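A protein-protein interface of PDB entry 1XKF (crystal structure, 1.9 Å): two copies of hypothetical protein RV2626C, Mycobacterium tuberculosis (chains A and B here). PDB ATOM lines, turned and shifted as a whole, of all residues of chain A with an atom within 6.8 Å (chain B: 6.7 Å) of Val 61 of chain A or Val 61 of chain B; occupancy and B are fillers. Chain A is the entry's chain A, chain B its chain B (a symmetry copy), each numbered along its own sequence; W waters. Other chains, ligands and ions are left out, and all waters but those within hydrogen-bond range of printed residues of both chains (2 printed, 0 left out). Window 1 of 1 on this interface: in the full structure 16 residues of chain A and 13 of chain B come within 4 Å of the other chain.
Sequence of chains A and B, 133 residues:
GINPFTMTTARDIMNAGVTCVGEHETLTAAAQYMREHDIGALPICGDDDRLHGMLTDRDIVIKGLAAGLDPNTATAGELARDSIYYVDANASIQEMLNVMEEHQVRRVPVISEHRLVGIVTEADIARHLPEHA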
ATOM      1  N   LEU A  27     -21.775 -30.413 -13.966  1.00  0.00           N
ATOM      2  CA  LEU A  27     -22.314 -30.294 -15.308  1.00  0.00           C
ATOM      3  C   LEU A  27     -21.831 -31.482 -16.137  1.00  0.00           C
ATOM      4  O   LEU A  27     -22.539 -31.954 -17.020  1.00  0.00           O
ATOM      5  CB  LEU A  27     -21.864 -28.971 -15.947  1.00  0.00           C
ATOM      6  CG  LEU A  27     -22.275 -27.697 -15.196  1.00  0.00           C
ATOM      7  CD1 LEU A  27     -21.828 -26.479 -15.981  1.00  0.00           C
ATOM      8  CD2 LEU A  27     -23.783 -27.675 -14.994  1.00  0.00           C
ATOM      9  N   THR A  28     -20.627 -31.967 -15.849  1.00  0.00           N
ATOM     10  CA  THR A  28     -20.096 -33.119 -16.574  1.00  0.00           C
ATOM     11  C   THR A  28     -20.961 -34.341 -16.272  1.00  0.00           C
ATOM     12  O   THR A  28     -21.241 -35.152 -17.158  1.00  0.00           O
ATOM     13  CB  THR A  28     -18.630 -33.417 -16.170  1.00  0.00           C
ATOM     14  OG1 THR A  28     -17.803 -32.301 -16.522  1.00  0.00           O
ATOM     15  CG2 THR A  28     -18.115 -34.657 -16.893  1.00  0.00           C
ATOM     16  N   ALA A  30     -24.106 -34.263 -15.427  1.00  0.00           N
ATOM     17  CA  ALA A  30     -25.364 -34.042 -16.139  1.00  0.00           C
ATOM     18  C   ALA A  30     -25.190 -34.419 -17.611  1.00  0.00           C
ATOM     19  O   ALA A  30     -26.051 -35.069 -18.200  1.00  0.00           O
ATOM     20  CB  ALA A  30     -25.784 -32.583 -16.025  1.00  0.00           C
ATOM     21  N   ALA A  31     -24.076 -33.996 -18.202  1.00  0.00           N
ATOM     22  CA  ALA A  31     -23.799 -34.301 -19.604  1.00  0.00           C
ATOM     23  C   ALA A  31     -23.818 -35.806 -19.825  1.00  0.00           C
ATOM     24  O   ALA A  31     -24.367 -36.288 -20.815  1.00  0.00           O
ATOM     25  CB  ALA A  31     -22.437 -33.730 -20.018  1.00  0.00           C
ATOM     26  N   GLN A  32     -23.216 -36.549 -18.900  1.00  0.00           N
ATOM     27  CA  GLN A  32     -23.181 -38.001 -19.009  1.00  0.00           C
ATOM     28  C   GLN A  32     -24.600 -38.575 -18.958  1.00  0.00           C
ATOM     29  O   GLN A  32     -24.927 -39.493 -19.704  1.00  0.00           O
ATOM     30  CB  GLN A  32     -22.325 -38.592 -17.887  1.00  0.00           C
ATOM     31  CG  GLN A  32     -20.900 -38.052 -17.875  1.00  0.00           C
ATOM     32  CD  GLN A  32     -20.070 -38.605 -16.733  1.00  0.00           C
ATOM     33  OE1 GLN A  32     -20.573 -38.813 -15.627  1.00  0.00           O
ATOM     34  NE2 GLN A  32     -18.787 -38.829 -16.990  1.00  0.00           N
ATOM     35  N   MET A  34     -27.299 -37.086 -19.900  1.00  0.00           N
ATOM     36  CA  MET A  34     -27.928 -36.729 -21.166  1.00  0.00           C
ATOM     37  C   MET A  34     -27.512 -37.670 -22.286  1.00  0.00           C
ATOM     38  O   MET A  34     -28.319 -37.993 -23.153  1.00  0.00           O
ATOM     39  CB  MET A  34     -27.586 -35.289 -21.544  1.00  0.00           C
ATOM     40  CG  MET A  34     -28.288 -34.263 -20.675  1.00  0.00           C
ATOM     41  SD  MET A  34     -27.807 -32.586 -21.093  1.00  0.00           S
ATOM     42  CE  MET A  34     -28.668 -31.656 -19.796  1.00  0.00           C
ATOM     43  N   ARG A  35     -26.257 -38.103 -22.278  1.00  0.00           N
ATOM     44  CA  ARG A  35     -25.802 -39.024 -23.308  1.00  0.00           C
ATOM     45  C   ARG A  35     -26.407 -40.392 -23.029  1.00  0.00           C
ATOM     46  O   ARG A  35     -26.960 -41.034 -23.917  1.00  0.00           O
ATOM     47  CB  ARG A  35     -24.281 -39.149 -23.313  1.00  0.00           C
ATOM     48  CG  ARG A  35     -23.791 -40.163 -24.339  1.00  0.00           C
ATOM     49  CD  ARG A  35     -22.278 -40.261 -24.388  1.00  0.00           C
ATOM     50  NE  ARG A  35     -21.730 -40.990 -23.253  1.00  0.00           N
ATOM     51  CZ  ARG A  35     -20.435 -41.255 -23.096  1.00  0.00           C
ATOM     52  NH1 ARG A  35     -19.559 -40.844 -24.004  1.00  0.00           N
ATOM     53  NH2 ARG A  35     -20.018 -41.936 -22.038  1.00  0.00           N
ATOM     54  N   THR A  56     -30.953 -27.958 -19.535  1.00  0.00           N
ATOM     55  CA  THR A  56     -30.901 -28.436 -20.915  1.00  0.00           C
ATOM     56  C   THR A  56     -29.455 -28.564 -21.387  1.00  0.00           C
ATOM     57  O   THR A  56     -28.538 -28.013 -20.765  1.00  0.00           O
ATOM     58  CB  THR A  56     -31.577 -27.452 -21.885  1.00  0.00           C
ATOM     59  OG1 THR A  56     -30.822 -26.234 -21.910  1.00  0.00           O
ATOM     60  CG2 THR A  56     -33.015 -27.158 -21.451  1.00  0.00           C
ATOM     61  N   ASP A  57     -29.244 -29.272 -22.493  1.00  0.00           N
ATOM     62  CA  ASP A  57     -27.889 -29.389 -23.007  1.00  0.00           C
ATOM     63  C   ASP A  57     -27.365 -28.007 -23.395  1.00  0.00           C
ATOM     64  O   ASP A  57     -26.204 -27.686 -23.134  1.00  0.00           O
ATOM     65  CB  ASP A  57     -27.792 -30.357 -24.208  1.00  0.00           C
ATOM     66  CG  ASP A  57     -28.958 -30.246 -25.190  1.00  0.00           C
ATOM     67  OD1 ASP A  57     -29.662 -29.214 -25.220  1.00  0.00           O
ATOM     68  OD2 ASP A  57     -29.154 -31.213 -25.960  1.00  0.00           O
ATOM     69  N   ARG A  58     -28.212 -27.176 -23.999  1.00  0.00           N
ATOM     70  CA  ARG A  58     -27.752 -25.844 -24.389  1.00  0.00           C
ATOM     71  C   ARG A  58     -27.391 -25.014 -23.159  1.00  0.00           C
ATOM     72  O   ARG A  58     -26.467 -24.202 -23.213  1.00  0.00           O
ATOM     73  CB  ARG A  58     -28.793 -25.108 -25.241  1.00  0.00           C
ATOM     74  CG  ARG A  58     -28.253 -23.786 -25.796  1.00  0.00           C
ATOM     75  CD  ARG A  58     -29.153 -23.160 -26.855  1.00  0.00           C
ATOM     76  NE  ARG A  58     -28.641 -21.863 -27.300  1.00  0.00           N
ATOM     77  CZ  ARG A  58     -27.603 -21.696 -28.117  1.00  0.00           C
ATOM     78  NH1 ARG A  58     -26.945 -22.748 -28.595  1.00  0.00           N
ATOM     79  NH2 ARG A  58     -27.222 -20.471 -28.458  1.00  0.00           N
ATOM     80  N   ASP A  59     -28.105 -25.219 -22.051  1.00  0.00           N
ATOM     81  CA  ASP A  59     -27.797 -24.489 -20.819  1.00  0.00           C
ATOM     82  C   ASP A  59     -26.335 -24.737 -20.446  1.00  0.00           C
ATOM     83  O   ASP A  59     -25.597 -23.809 -20.114  1.00  0.00           O
ATOM     84  CB  ASP A  59     -28.665 -24.960 -19.641  1.00  0.00           C
ATOM     85  CG  ASP A  59     -30.077 -24.417 -19.684  1.00  0.00           C
ATOM     86  OD1 ASP A  59     -30.300 -23.353 -20.300  1.00  0.00           O
ATOM     87  OD2 ASP A  59     -30.967 -25.051 -19.077  1.00  0.00           O
ATOM     88  N   ILE A  60     -25.929 -26.001 -20.485  1.00  0.00           N
ATOM     89  CA  ILE A  60     -24.557 -26.364 -20.150  1.00  0.00           C
ATOM     90  C   ILE A  60     -23.566 -25.620 -21.047  1.00  0.00           C
ATOM     91  O   ILE A  60     -22.546 -25.124 -20.580  1.00  0.00           O
ATOM     92  CB  ILE A  60     -24.338 -27.893 -20.287  1.00  0.00           C
ATOM     93  CG1 ILE A  60     -25.169 -28.624 -19.226  1.00  0.00           C
ATOM     94  CG2 ILE A  60     -22.848 -28.235 -20.119  1.00  0.00           C
ATOM     95  CD1 ILE A  60     -25.066 -30.118 -19.280  1.00  0.00           C
ATOM     96  N   VAL A  61     -23.882 -25.533 -22.332  1.00  0.00           N
ATOM     97  CA  VAL A  61     -23.017 -24.860 -23.293  1.00  0.00           C
ATOM     98  C   VAL A  61     -22.975 -23.343 -23.105  1.00  0.00           C
ATOM     99  O   VAL A  61     -21.897 -22.742 -23.048  1.00  0.00           O
ATOM    100  CB  VAL A  61     -23.474 -25.163 -24.748  1.00  0.00           C
ATOM    101  CG1 VAL A  61     -22.634 -24.373 -25.745  1.00  0.00           C
ATOM    102  CG2 VAL A  61     -23.364 -26.665 -25.031  1.00  0.00           C
ATOM    103  N   ILE A  62     -24.152 -22.735 -22.999  1.00  0.00           N
ATOM    104  CA  ILE A  62     -24.275 -21.285 -22.880  1.00  0.00           C
ATOM    105  C   ILE A  62     -24.102 -20.688 -21.485  1.00  0.00           C
ATOM    106  O   ILE A  62     -23.405 -19.688 -21.325  1.00  0.00           O
ATOM    107  CB  ILE A  62     -25.635 -20.819 -23.448  1.00  0.00           C
ATOM    108  CG1 ILE A  62     -25.811 -21.348 -24.876  1.00  0.00           C
ATOM    109  CG2 ILE A  62     -25.726 -19.296 -23.422  1.00  0.00           C
ATOM    110  CD1 ILE A  62     -24.768 -20.854 -25.871  1.00  0.00           C
ATOM    111  N   LYS A  63     -24.743 -21.281 -20.483  1.00  0.00           N
ATOM    112  CA  LYS A  63     -24.632 -20.773 -19.116  1.00  0.00           C
ATOM    113  C   LYS A  63     -23.427 -21.391 -18.416  1.00  0.00           C
ATOM    114  O   LYS A  63     -22.988 -20.910 -17.376  1.00  0.00           O
ATOM    115  CB  LYS A  63     -25.901 -21.091 -18.320  1.00  0.00           C
ATOM    116  CG  LYS A  63     -27.170 -20.424 -18.843  1.00  0.00           C
ATOM    117  CD  LYS A  63     -28.375 -20.824 -17.997  1.00  0.00           C
ATOM    118  CE  LYS A  63     -29.642 -20.121 -18.447  1.00  0.00           C
ATOM    119  NZ  LYS A  63     -30.825 -20.556 -17.639  1.00  0.00           N
ATOM    120  N   GLY A  64     -22.892 -22.460 -18.998  1.00  0.00           N
ATOM    121  CA  GLY A  64     -21.746 -23.121 -18.407  1.00  0.00           C
ATOM    122  C   GLY A  64     -20.434 -22.793 -19.098  1.00  0.00           C
ATOM    123  O   GLY A  64     -19.695 -21.910 -18.661  1.00  0.00           O
ATOM    124  N   LEU A  65     -20.150 -23.494 -20.191  1.00  0.00           N
ATOM    125  CA  LEU A  65     -18.905 -23.290 -20.921  1.00  0.00           C
ATOM    126  C   LEU A  65     -18.678 -21.855 -21.406  1.00  0.00           C
ATOM    127  O   LEU A  65     -17.587 -21.307 -21.238  1.00  0.00           O
ATOM    128  CB  LEU A  65     -18.832 -24.265 -22.103  1.00  0.00           C
ATOM    129  CG  LEU A  65     -19.022 -25.747 -21.748  1.00  0.00           C
ATOM    130  CD1 LEU A  65     -18.881 -26.592 -23.003  1.00  0.00           C
ATOM    131  CD2 LEU A  65     -18.003 -26.176 -20.700  1.00  0.00           C
ATOM    132  N   ALA A  66     -19.700 -21.250 -22.001  1.00  0.00           N
ATOM    133  CA  ALA A  66     -19.584 -19.887 -22.511  1.00  0.00           C
ATOM    134  C   ALA A  66     -19.389 -18.858 -21.399  1.00  0.00           C
ATOM    135  O   ALA A  66     -18.854 -17.776 -21.639  1.00  0.00           O
ATOM    136  CB  ALA A  66     -20.821 -19.525 -23.343  1.00  0.00           C
ATOM    137  N   ALA A  67     -19.828 -19.193 -20.189  1.00  0.00           N
ATOM    138  CA  ALA A  67     -19.690 -18.289 -19.051  1.00  0.00           C
ATOM    139  C   ALA A  67     -18.353 -18.496 -18.345  1.00  0.00           C
ATOM    140  O   ALA A  67     -18.081 -17.879 -17.315  1.00  0.00           O
ATOM    141  CB  ALA A  67     -20.838 -18.503 -18.073  1.00  0.00           C
ATOM    142  N   LEU A  79     -26.887 -23.708 -12.073  1.00  0.00           N
ATOM    143  CA  LEU A  79     -27.433 -23.254 -13.349  1.00  0.00           C
ATOM    144  C   LEU A  79     -28.955 -23.366 -13.361  1.00  0.00           C
ATOM    145  O   LEU A  79     -29.609 -22.934 -14.309  1.00  0.00           O
ATOM    146  CB  LEU A  79     -26.856 -24.067 -14.510  1.00  0.00           C
ATOM    147  CG  LEU A  79     -25.611 -23.521 -15.215  1.00  0.00           C
ATOM    148  CD1 LEU A  79     -24.469 -23.365 -14.224  1.00  0.00           C
ATOM    149  CD2 LEU A  79     -25.221 -24.465 -16.338  1.00  0.00           C
ATOM    150  N   LEU B  27     -13.568 -26.294 -27.993  1.00  0.00           N
ATOM    151  CA  LEU B  27     -14.991 -26.438 -27.731  1.00  0.00           C
ATOM    152  C   LEU B  27     -15.476 -25.246 -26.902  1.00  0.00           C
ATOM    153  O   LEU B  27     -16.607 -24.795 -27.054  1.00  0.00           O
ATOM    154  CB  LEU B  27     -15.267 -27.760 -26.999  1.00  0.00           C
ATOM    155  CG  LEU B  27     -14.881 -29.011 -27.802  1.00  0.00           C
ATOM    156  CD1 LEU B  27     -15.317 -30.271 -27.063  1.00  0.00           C
ATOM    157  CD2 LEU B  27     -15.536 -28.950 -29.175  1.00  0.00           C
ATOM    158  N   THR B  28     -14.615 -24.730 -26.031  1.00  0.00           N
ATOM    159  CA  THR B  28     -14.980 -23.576 -25.212  1.00  0.00           C
ATOM    160  C   THR B  28     -15.184 -22.365 -26.117  1.00  0.00           C
ATOM    161  O   THR B  28     -16.140 -21.608 -25.947  1.00  0.00           O
ATOM    162  CB  THR B  28     -13.889 -23.241 -24.180  1.00  0.00           C
ATOM    163  OG1 THR B  28     -13.799 -24.302 -23.226  1.00  0.00           O
ATOM    164  CG2 THR B  28     -14.213 -21.933 -23.462  1.00  0.00           C
ATOM    165  N   ALA B  30     -15.987 -22.453 -29.218  1.00  0.00           N
ATOM    166  CA  ALA B  30     -17.178 -22.700 -30.031  1.00  0.00           C
ATOM    167  C   ALA B  30     -18.419 -22.389 -29.202  1.00  0.00           C
ATOM    168  O   ALA B  30     -19.418 -21.896 -29.730  1.00  0.00           O
ATOM    169  CB  ALA B  30     -17.211 -24.150 -30.513  1.00  0.00           C
ATOM    170  N   ALA B  31     -18.356 -22.680 -27.904  1.00  0.00           N
ATOM    171  CA  ALA B  31     -19.479 -22.396 -27.005  1.00  0.00           C
ATOM    172  C   ALA B  31     -19.656 -20.882 -26.909  1.00  0.00           C
ATOM    173  O   ALA B  31     -20.775 -20.365 -26.964  1.00  0.00           O
ATOM    174  CB  ALA B  31     -19.213 -22.972 -25.615  1.00  0.00           C
ATOM    175  N   GLN B  32     -18.543 -20.173 -26.756  1.00  0.00           N
ATOM    176  CA  GLN B  32     -18.592 -18.719 -26.672  1.00  0.00           C
ATOM    177  C   GLN B  32     -19.173 -18.159 -27.971  1.00  0.00           C
ATOM    178  O   GLN B  32     -19.954 -17.200 -27.955  1.00  0.00           O
ATOM    179  CB  GLN B  32     -17.186 -18.161 -26.426  1.00  0.00           C
ATOM    180  CG  GLN B  32     -16.637 -18.502 -25.046  1.00  0.00           C
ATOM    181  CD  GLN B  32     -15.159 -18.190 -24.896  1.00  0.00           C
ATOM    182  OE1 GLN B  32     -14.665 -18.012 -23.785  1.00  0.00           O
ATOM    183  NE2 GLN B  32     -14.444 -18.141 -26.013  1.00  0.00           N
ATOM    184  N   MET B  34     -21.277 -19.682 -30.008  1.00  0.00           N
ATOM    185  CA  MET B  34     -22.713 -19.969 -30.029  1.00  0.00           C
ATOM    186  C   MET B  34     -23.496 -18.966 -29.181  1.00  0.00           C
ATOM    187  O   MET B  34     -24.616 -18.585 -29.537  1.00  0.00           O
ATOM    188  CB  MET B  34     -22.979 -21.393 -29.539  1.00  0.00           C
ATOM    189  CG  MET B  34     -22.469 -22.459 -30.491  1.00  0.00           C
ATOM    190  SD  MET B  34     -22.727 -24.113 -29.850  1.00  0.00           S
ATOM    191  CE  MET B  34     -21.884 -25.102 -31.126  1.00  0.00           C
ATOM    192  N   ARG B  35     -22.916 -18.543 -28.060  1.00  0.00           N
ATOM    193  CA  ARG B  35     -23.580 -17.562 -27.202  1.00  0.00           C
ATOM    194  C   ARG B  35     -23.539 -16.187 -27.867  1.00  0.00           C
ATOM    195  O   ARG B  35     -24.556 -15.503 -27.985  1.00  0.00           O
ATOM    196  CB  ARG B  35     -22.897 -17.460 -25.837  1.00  0.00           C
ATOM    197  CG  ARG B  35     -23.537 -16.399 -24.935  1.00  0.00           C
ATOM    198  CD  ARG B  35     -22.888 -16.305 -23.559  1.00  0.00           C
ATOM    199  NE  ARG B  35     -21.512 -15.822 -23.613  1.00  0.00           N
ATOM    200  CZ  ARG B  35     -20.787 -15.525 -22.538  1.00  0.00           C
ATOM    201  NH1 ARG B  35     -21.310 -15.659 -21.324  1.00  0.00           N
ATOM    202  NH2 ARG B  35     -19.536 -15.099 -22.674  1.00  0.00           N
ATOM    203  N   THR B  56     -22.834 -29.045 -33.263  1.00  0.00           N
ATOM    204  CA  THR B  56     -23.998 -28.489 -32.582  1.00  0.00           C
ATOM    205  C   THR B  56     -23.725 -28.295 -31.097  1.00  0.00           C
ATOM    206  O   THR B  56     -22.763 -28.848 -30.558  1.00  0.00           O
ATOM    207  CB  THR B  56     -25.207 -29.423 -32.704  1.00  0.00           C
ATOM    208  OG1 THR B  56     -24.905 -30.671 -32.063  1.00  0.00           O
ATOM    209  CG2 THR B  56     -25.541 -29.674 -34.168  1.00  0.00           C
ATOM    210  N   ASP B  57     -24.567 -27.505 -30.431  1.00  0.00           N
ATOM    211  CA  ASP B  57     -24.387 -27.312 -29.007  1.00  0.00           C
ATOM    212  C   ASP B  57     -24.504 -28.670 -28.326  1.00  0.00           C
ATOM    213  O   ASP B  57     -23.735 -28.983 -27.414  1.00  0.00           O
ATOM    214  CB  ASP B  57     -25.413 -26.321 -28.421  1.00  0.00           C
ATOM    215  CG  ASP B  57     -26.814 -26.483 -28.997  1.00  0.00           C
ATOM    216  OD1 ASP B  57     -27.167 -27.576 -29.485  1.00  0.00           O
ATOM    217  OD2 ASP B  57     -27.578 -25.498 -28.936  1.00  0.00           O
ATOM    218  N   ARG B  58     -25.437 -29.495 -28.786  1.00  0.00           N
ATOM    219  CA  ARG B  58     -25.600 -30.816 -28.179  1.00  0.00           C
ATOM    220  C   ARG B  58     -24.340 -31.666 -28.348  1.00  0.00           C
ATOM    221  O   ARG B  58     -23.974 -32.421 -27.450  1.00  0.00           O
ATOM    222  CB  ARG B  58     -26.806 -31.553 -28.769  1.00  0.00           C
ATOM    223  CG  ARG B  58     -27.093 -32.873 -28.053  1.00  0.00           C
ATOM    224  CD  ARG B  58     -28.384 -33.530 -28.528  1.00  0.00           C
ATOM    225  NE  ARG B  58     -28.554 -34.861 -27.946  1.00  0.00           N
ATOM    226  CZ  ARG B  58     -28.750 -35.103 -26.651  1.00  0.00           C
ATOM    227  NH1 ARG B  58     -28.811 -34.100 -25.779  1.00  0.00           N
ATOM    228  NH2 ARG B  58     -28.881 -36.351 -26.223  1.00  0.00           N
ATOM    229  N   ASP B  59     -23.676 -31.549 -29.497  1.00  0.00           N
ATOM    230  CA  ASP B  59     -22.449 -32.316 -29.736  1.00  0.00           C
ATOM    231  C   ASP B  59     -21.402 -32.021 -28.667  1.00  0.00           C
ATOM    232  O   ASP B  59     -20.744 -32.925 -28.157  1.00  0.00           O
ATOM    233  CB  ASP B  59     -21.826 -31.978 -31.098  1.00  0.00           C
ATOM    234  CG  ASP B  59     -22.576 -32.591 -32.261  1.00  0.00           C
ATOM    235  OD1 ASP B  59     -23.248 -33.628 -32.072  1.00  0.00           O
ATOM    236  OD2 ASP B  59     -22.472 -32.039 -33.375  1.00  0.00           O
ATOM    237  N   ILE B  60     -21.231 -30.743 -28.352  1.00  0.00           N
ATOM    238  CA  ILE B  60     -20.253 -30.343 -27.354  1.00  0.00           C
ATOM    239  C   ILE B  60     -20.507 -31.043 -26.028  1.00  0.00           C
ATOM    240  O   ILE B  60     -19.572 -31.473 -25.347  1.00  0.00           O
ATOM    241  CB  ILE B  60     -20.275 -28.819 -27.146  1.00  0.00           C
ATOM    242  CG1 ILE B  60     -19.738 -28.125 -28.407  1.00  0.00           C
ATOM    243  CG2 ILE B  60     -19.439 -28.446 -25.926  1.00  0.00           C
ATOM    244  CD1 ILE B  60     -19.839 -26.612 -28.378  1.00  0.00           C
ATOM    245  N   VAL B  61     -21.778 -31.163 -25.668  1.00  0.00           N
ATOM    246  CA  VAL B  61     -22.155 -31.811 -24.419  1.00  0.00           C
ATOM    247  C   VAL B  61     -22.008 -33.332 -24.483  1.00  0.00           C
ATOM    248  O   VAL B  61     -21.390 -33.942 -23.605  1.00  0.00           O
ATOM    249  CB  VAL B  61     -23.621 -31.478 -24.050  1.00  0.00           C
ATOM    250  CG1 VAL B  61     -24.033 -32.243 -22.789  1.00  0.00           C
ATOM    251  CG2 VAL B  61     -23.777 -29.977 -23.843  1.00  0.00           C
ATOM    252  N   ILE B  62     -22.566 -33.928 -25.533  1.00  0.00           N
ATOM    253  CA  ILE B  62     -22.566 -35.379 -25.718  1.00  0.00           C
ATOM    254  C   ILE B  62     -21.281 -36.021 -26.237  1.00  0.00           C
ATOM    255  O   ILE B  62     -20.854 -37.057 -25.730  1.00  0.00           O
ATOM    256  CB  ILE B  62     -23.714 -35.800 -26.658  1.00  0.00           C
ATOM    257  CG1 ILE B  62     -25.048 -35.295 -26.101  1.00  0.00           C
ATOM    258  CG2 ILE B  62     -23.737 -37.315 -26.812  1.00  0.00           C
ATOM    259  CD1 ILE B  62     -25.372 -35.830 -24.719  1.00  0.00           C
ATOM    260  N   LYS B  63     -20.684 -35.431 -27.262  1.00  0.00           N
ATOM    261  CA  LYS B  63     -19.460 -35.984 -27.821  1.00  0.00           C
ATOM    262  C   LYS B  63     -18.247 -35.392 -27.128  1.00  0.00           C
ATOM    263  O   LYS B  63     -17.146 -35.934 -27.209  1.00  0.00           O
ATOM    264  CB  LYS B  63     -19.394 -35.709 -29.322  1.00  0.00           C
ATOM    265  CG  LYS B  63     -20.455 -36.447 -30.130  1.00  0.00           C
ATOM    266  CD  LYS B  63     -20.317 -36.163 -31.618  1.00  0.00           C
ATOM    267  CE  LYS B  63     -21.350 -36.939 -32.420  1.00  0.00           C
ATOM    268  NZ  LYS B  63     -21.288 -36.596 -33.869  1.00  0.00           N
ATOM    269  N   GLY B  64     -18.459 -34.277 -26.438  1.00  0.00           N
ATOM    270  CA  GLY B  64     -17.365 -33.628 -25.743  1.00  0.00           C
ATOM    271  C   GLY B  64     -17.333 -33.945 -24.261  1.00  0.00           C
ATOM    272  O   GLY B  64     -16.617 -34.848 -23.830  1.00  0.00           O
ATOM    273  N   LEU B  65     -18.124 -33.213 -23.483  1.00  0.00           N
ATOM    274  CA  LEU B  65     -18.168 -33.395 -22.037  1.00  0.00           C
ATOM    275  C   LEU B  65     -18.497 -34.822 -21.597  1.00  0.00           C
ATOM    276  O   LEU B  65     -17.820 -35.379 -20.733  1.00  0.00           O
ATOM    277  CB  LEU B  65     -19.178 -32.424 -21.414  1.00  0.00           C
ATOM    278  CG  LEU B  65     -18.972 -30.931 -21.700  1.00  0.00           C
ATOM    279  CD1 LEU B  65     -19.934 -30.125 -20.836  1.00  0.00           C
ATOM    280  CD2 LEU B  65     -17.537 -30.522 -21.407  1.00  0.00           C
ATOM    281  N   ALA B  66     -19.536 -35.405 -22.188  1.00  0.00           N
ATOM    282  CA  ALA B  66     -19.948 -36.761 -21.837  1.00  0.00           C
ATOM    283  C   ALA B  66     -18.896 -37.805 -22.202  1.00  0.00           C
ATOM    284  O   ALA B  66     -18.889 -38.899 -21.638  1.00  0.00           O
ATOM    285  CB  ALA B  66     -21.268 -37.100 -22.511  1.00  0.00           C
ATOM    286  N   ALA B  67     -18.015 -37.473 -23.143  1.00  0.00           N
ATOM    287  CA  ALA B  67     -16.971 -38.407 -23.559  1.00  0.00           C
ATOM    288  C   ALA B  67     -15.667 -38.173 -22.802  1.00  0.00           C
ATOM    289  O   ALA B  67     -14.641 -38.778 -23.116  1.00  0.00           O
ATOM    290  CB  ALA B  67     -16.735 -38.290 -25.059  1.00  0.00           C
ATOM    291  N   LEU B  79     -14.677 -32.970 -33.345  1.00  0.00           N
ATOM    292  CA  LEU B  79     -16.046 -33.445 -33.169  1.00  0.00           C
ATOM    293  C   LEU B  79     -16.872 -33.349 -34.455  1.00  0.00           C
ATOM    294  O   LEU B  79     -17.670 -34.237 -34.757  1.00  0.00           O
ATOM    295  CB  LEU B  79     -16.744 -32.668 -32.039  1.00  0.00           C
ATOM    296  CG  LEU B  79     -16.501 -33.113 -30.588  1.00  0.00           C
ATOM    297  CD1 LEU B  79     -15.035 -32.973 -30.231  1.00  0.00           C
ATOM    298  CD2 LEU B  79     -17.354 -32.264 -29.646  1.00  0.00           C
HETATM  299  O   HOH W   1     -20.087 -39.455 -26.448  1.00  0.00           O
HETATM  300  O   HOH W   2     -23.605 -17.186 -20.418  1.00  0.00           O
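Printed residues of chain A that touch a printed residue of chain B: Thr 28, Ala 31, Met 34, Arg 35, Asp 57, Arg 58, Ile 60, Val 61, Ile 62, Leu 65, Ala 66 and Ala 67. Hydrophobic or aromatic side chains of chain A that line the printed part of chain B: Ala 31, Met 34, Ile 60, Val 61, Ile 62, Leu 65 and Ala 66. Among the printed residues, 23 pairs touch across the chains.
Arg 35 of chain A touches Ala 67 of chain B, and with the chains exchanged Ala 67 of chain A touches Arg 35 of chain B. Positions printed for both chains: 27, 28, 30, 31, 32, 34, 35, 56, 57, 58, 59, 60, 61, 62, 63, 64, 65, 66, 67 and 79.
N of Ala 66 of chain A sits at hydrogen-bond distance from O of Val 61 of chain A (2.9 Å). O of Val 61 of chain B lies within hydrogen-bond range of N of Ala 66 of chain B (2.8 Å). The backbone NH of Arg 58 of chain A sits close to the side-chain hydroxyl of Thr 56 of chain A (3.5 Å).
Among the printed residues, merely in contact across the chains: Val 61 of chain A with Asp 57 of chain B (3.3 Å), Asp 57 of chain A with Val 61 of chain B (3.4 Å), Arg 35 of chain A with Ile 62 of chain B (3.5 Å), Leu 65 of chain A with Ile 60 of chain B (3.5 Å), Ala 31 of chain A with Val 61 of chain B (3.5 Å), Met 34 of chain A with Arg 58 of chain B (3.5 Å), Val 61 of chain A with Val 61 of chain B (3.5 Å), Ile 60 of chain A with Leu 65 of chain B (3.5 Å), Arg 35 of chain A with Ala 67 of chain B (3.6 Å), Ala 31 of chain A with Ala 66 of chain B (3.6 Å), Ile 62 of chain A with Arg 35 of chain B (3.7 Å), Val 61 of chain A with Ala 31 of chain B (3.7 Å), Ala 66 of chain A with Ala 31 of chain B (3.7 Å), Met 34 of chain A with Ile 62 of chain B (3.7 Å), Leu 65 of chain A with Ala 31 of chain B (3.8 Å), Ala 31 of chain A with Leu 65 of chain B (3.8 Å), Ala 67 of chain A with Arg 35 of chain B (3.8 Å) and Thr 28 of chain A with Leu 65 of chain B (3.9 Å).
Water W1 lies within hydrogen-bond range of O of Ile 62 of chain B and NH1 of Arg 35 of chain A. Water W2 lies within hydrogen-bond range of the backbone carbonyl oxygen (O) of Ile 62 of chain A (2.7 Å) and the guanidinium group (NH1) of Arg 35 of chain B (2.9 Å).
Gln 32 of chain A touches none of the printed residues of chain B. Printed residues of chain B within 4 Å of Asp 57 of chain A: Arg 58 (2.9 Å) and Val 61 (3.4 Å). Of chain B, only Ala 31, Asp 57 and Val 61 come within 4 Å of Val 61 of chain A. Printed residues of chain B within 4 Å of Leu 65 of chain A: Ala 31 and Ile 60. Val 61 of chain B touches three residues of chain A. The nearest printed residue of chain A that does not touch Val 61 of chain B is Met 34 of chain A (4.2 Å). The nearest printed residue of chain B that does not touch Ala 31 of chain A is Ile 62 of chain B (4.1 Å).
The guanidinium group of Arg 35 of chain A sits at hydrogen-bond distance from the backbone carbonyl oxygen of Ala 66 of chain B, 3.1 Å away. The backbone carbonyl oxygen of Ala 66 of chain A lies within hydrogen-bond range of the guanidinium group of Arg 35 of chain B, 3.0 Å away. The guanidinium group (NH1) of Arg 58 of chain B lies within salt-bridge range of the side-chain carboxylate (OD2) of Asp 57 of chain A, 2.9 Å away. NH2 of Arg 58 of chain A is in hydrogen-bond range of O of Met 34 of chain B (3.4 Å). NH1 of Arg 58 of chain A is in salt-bridge range of OD2 of Asp 57 of chain B (2.8 Å).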
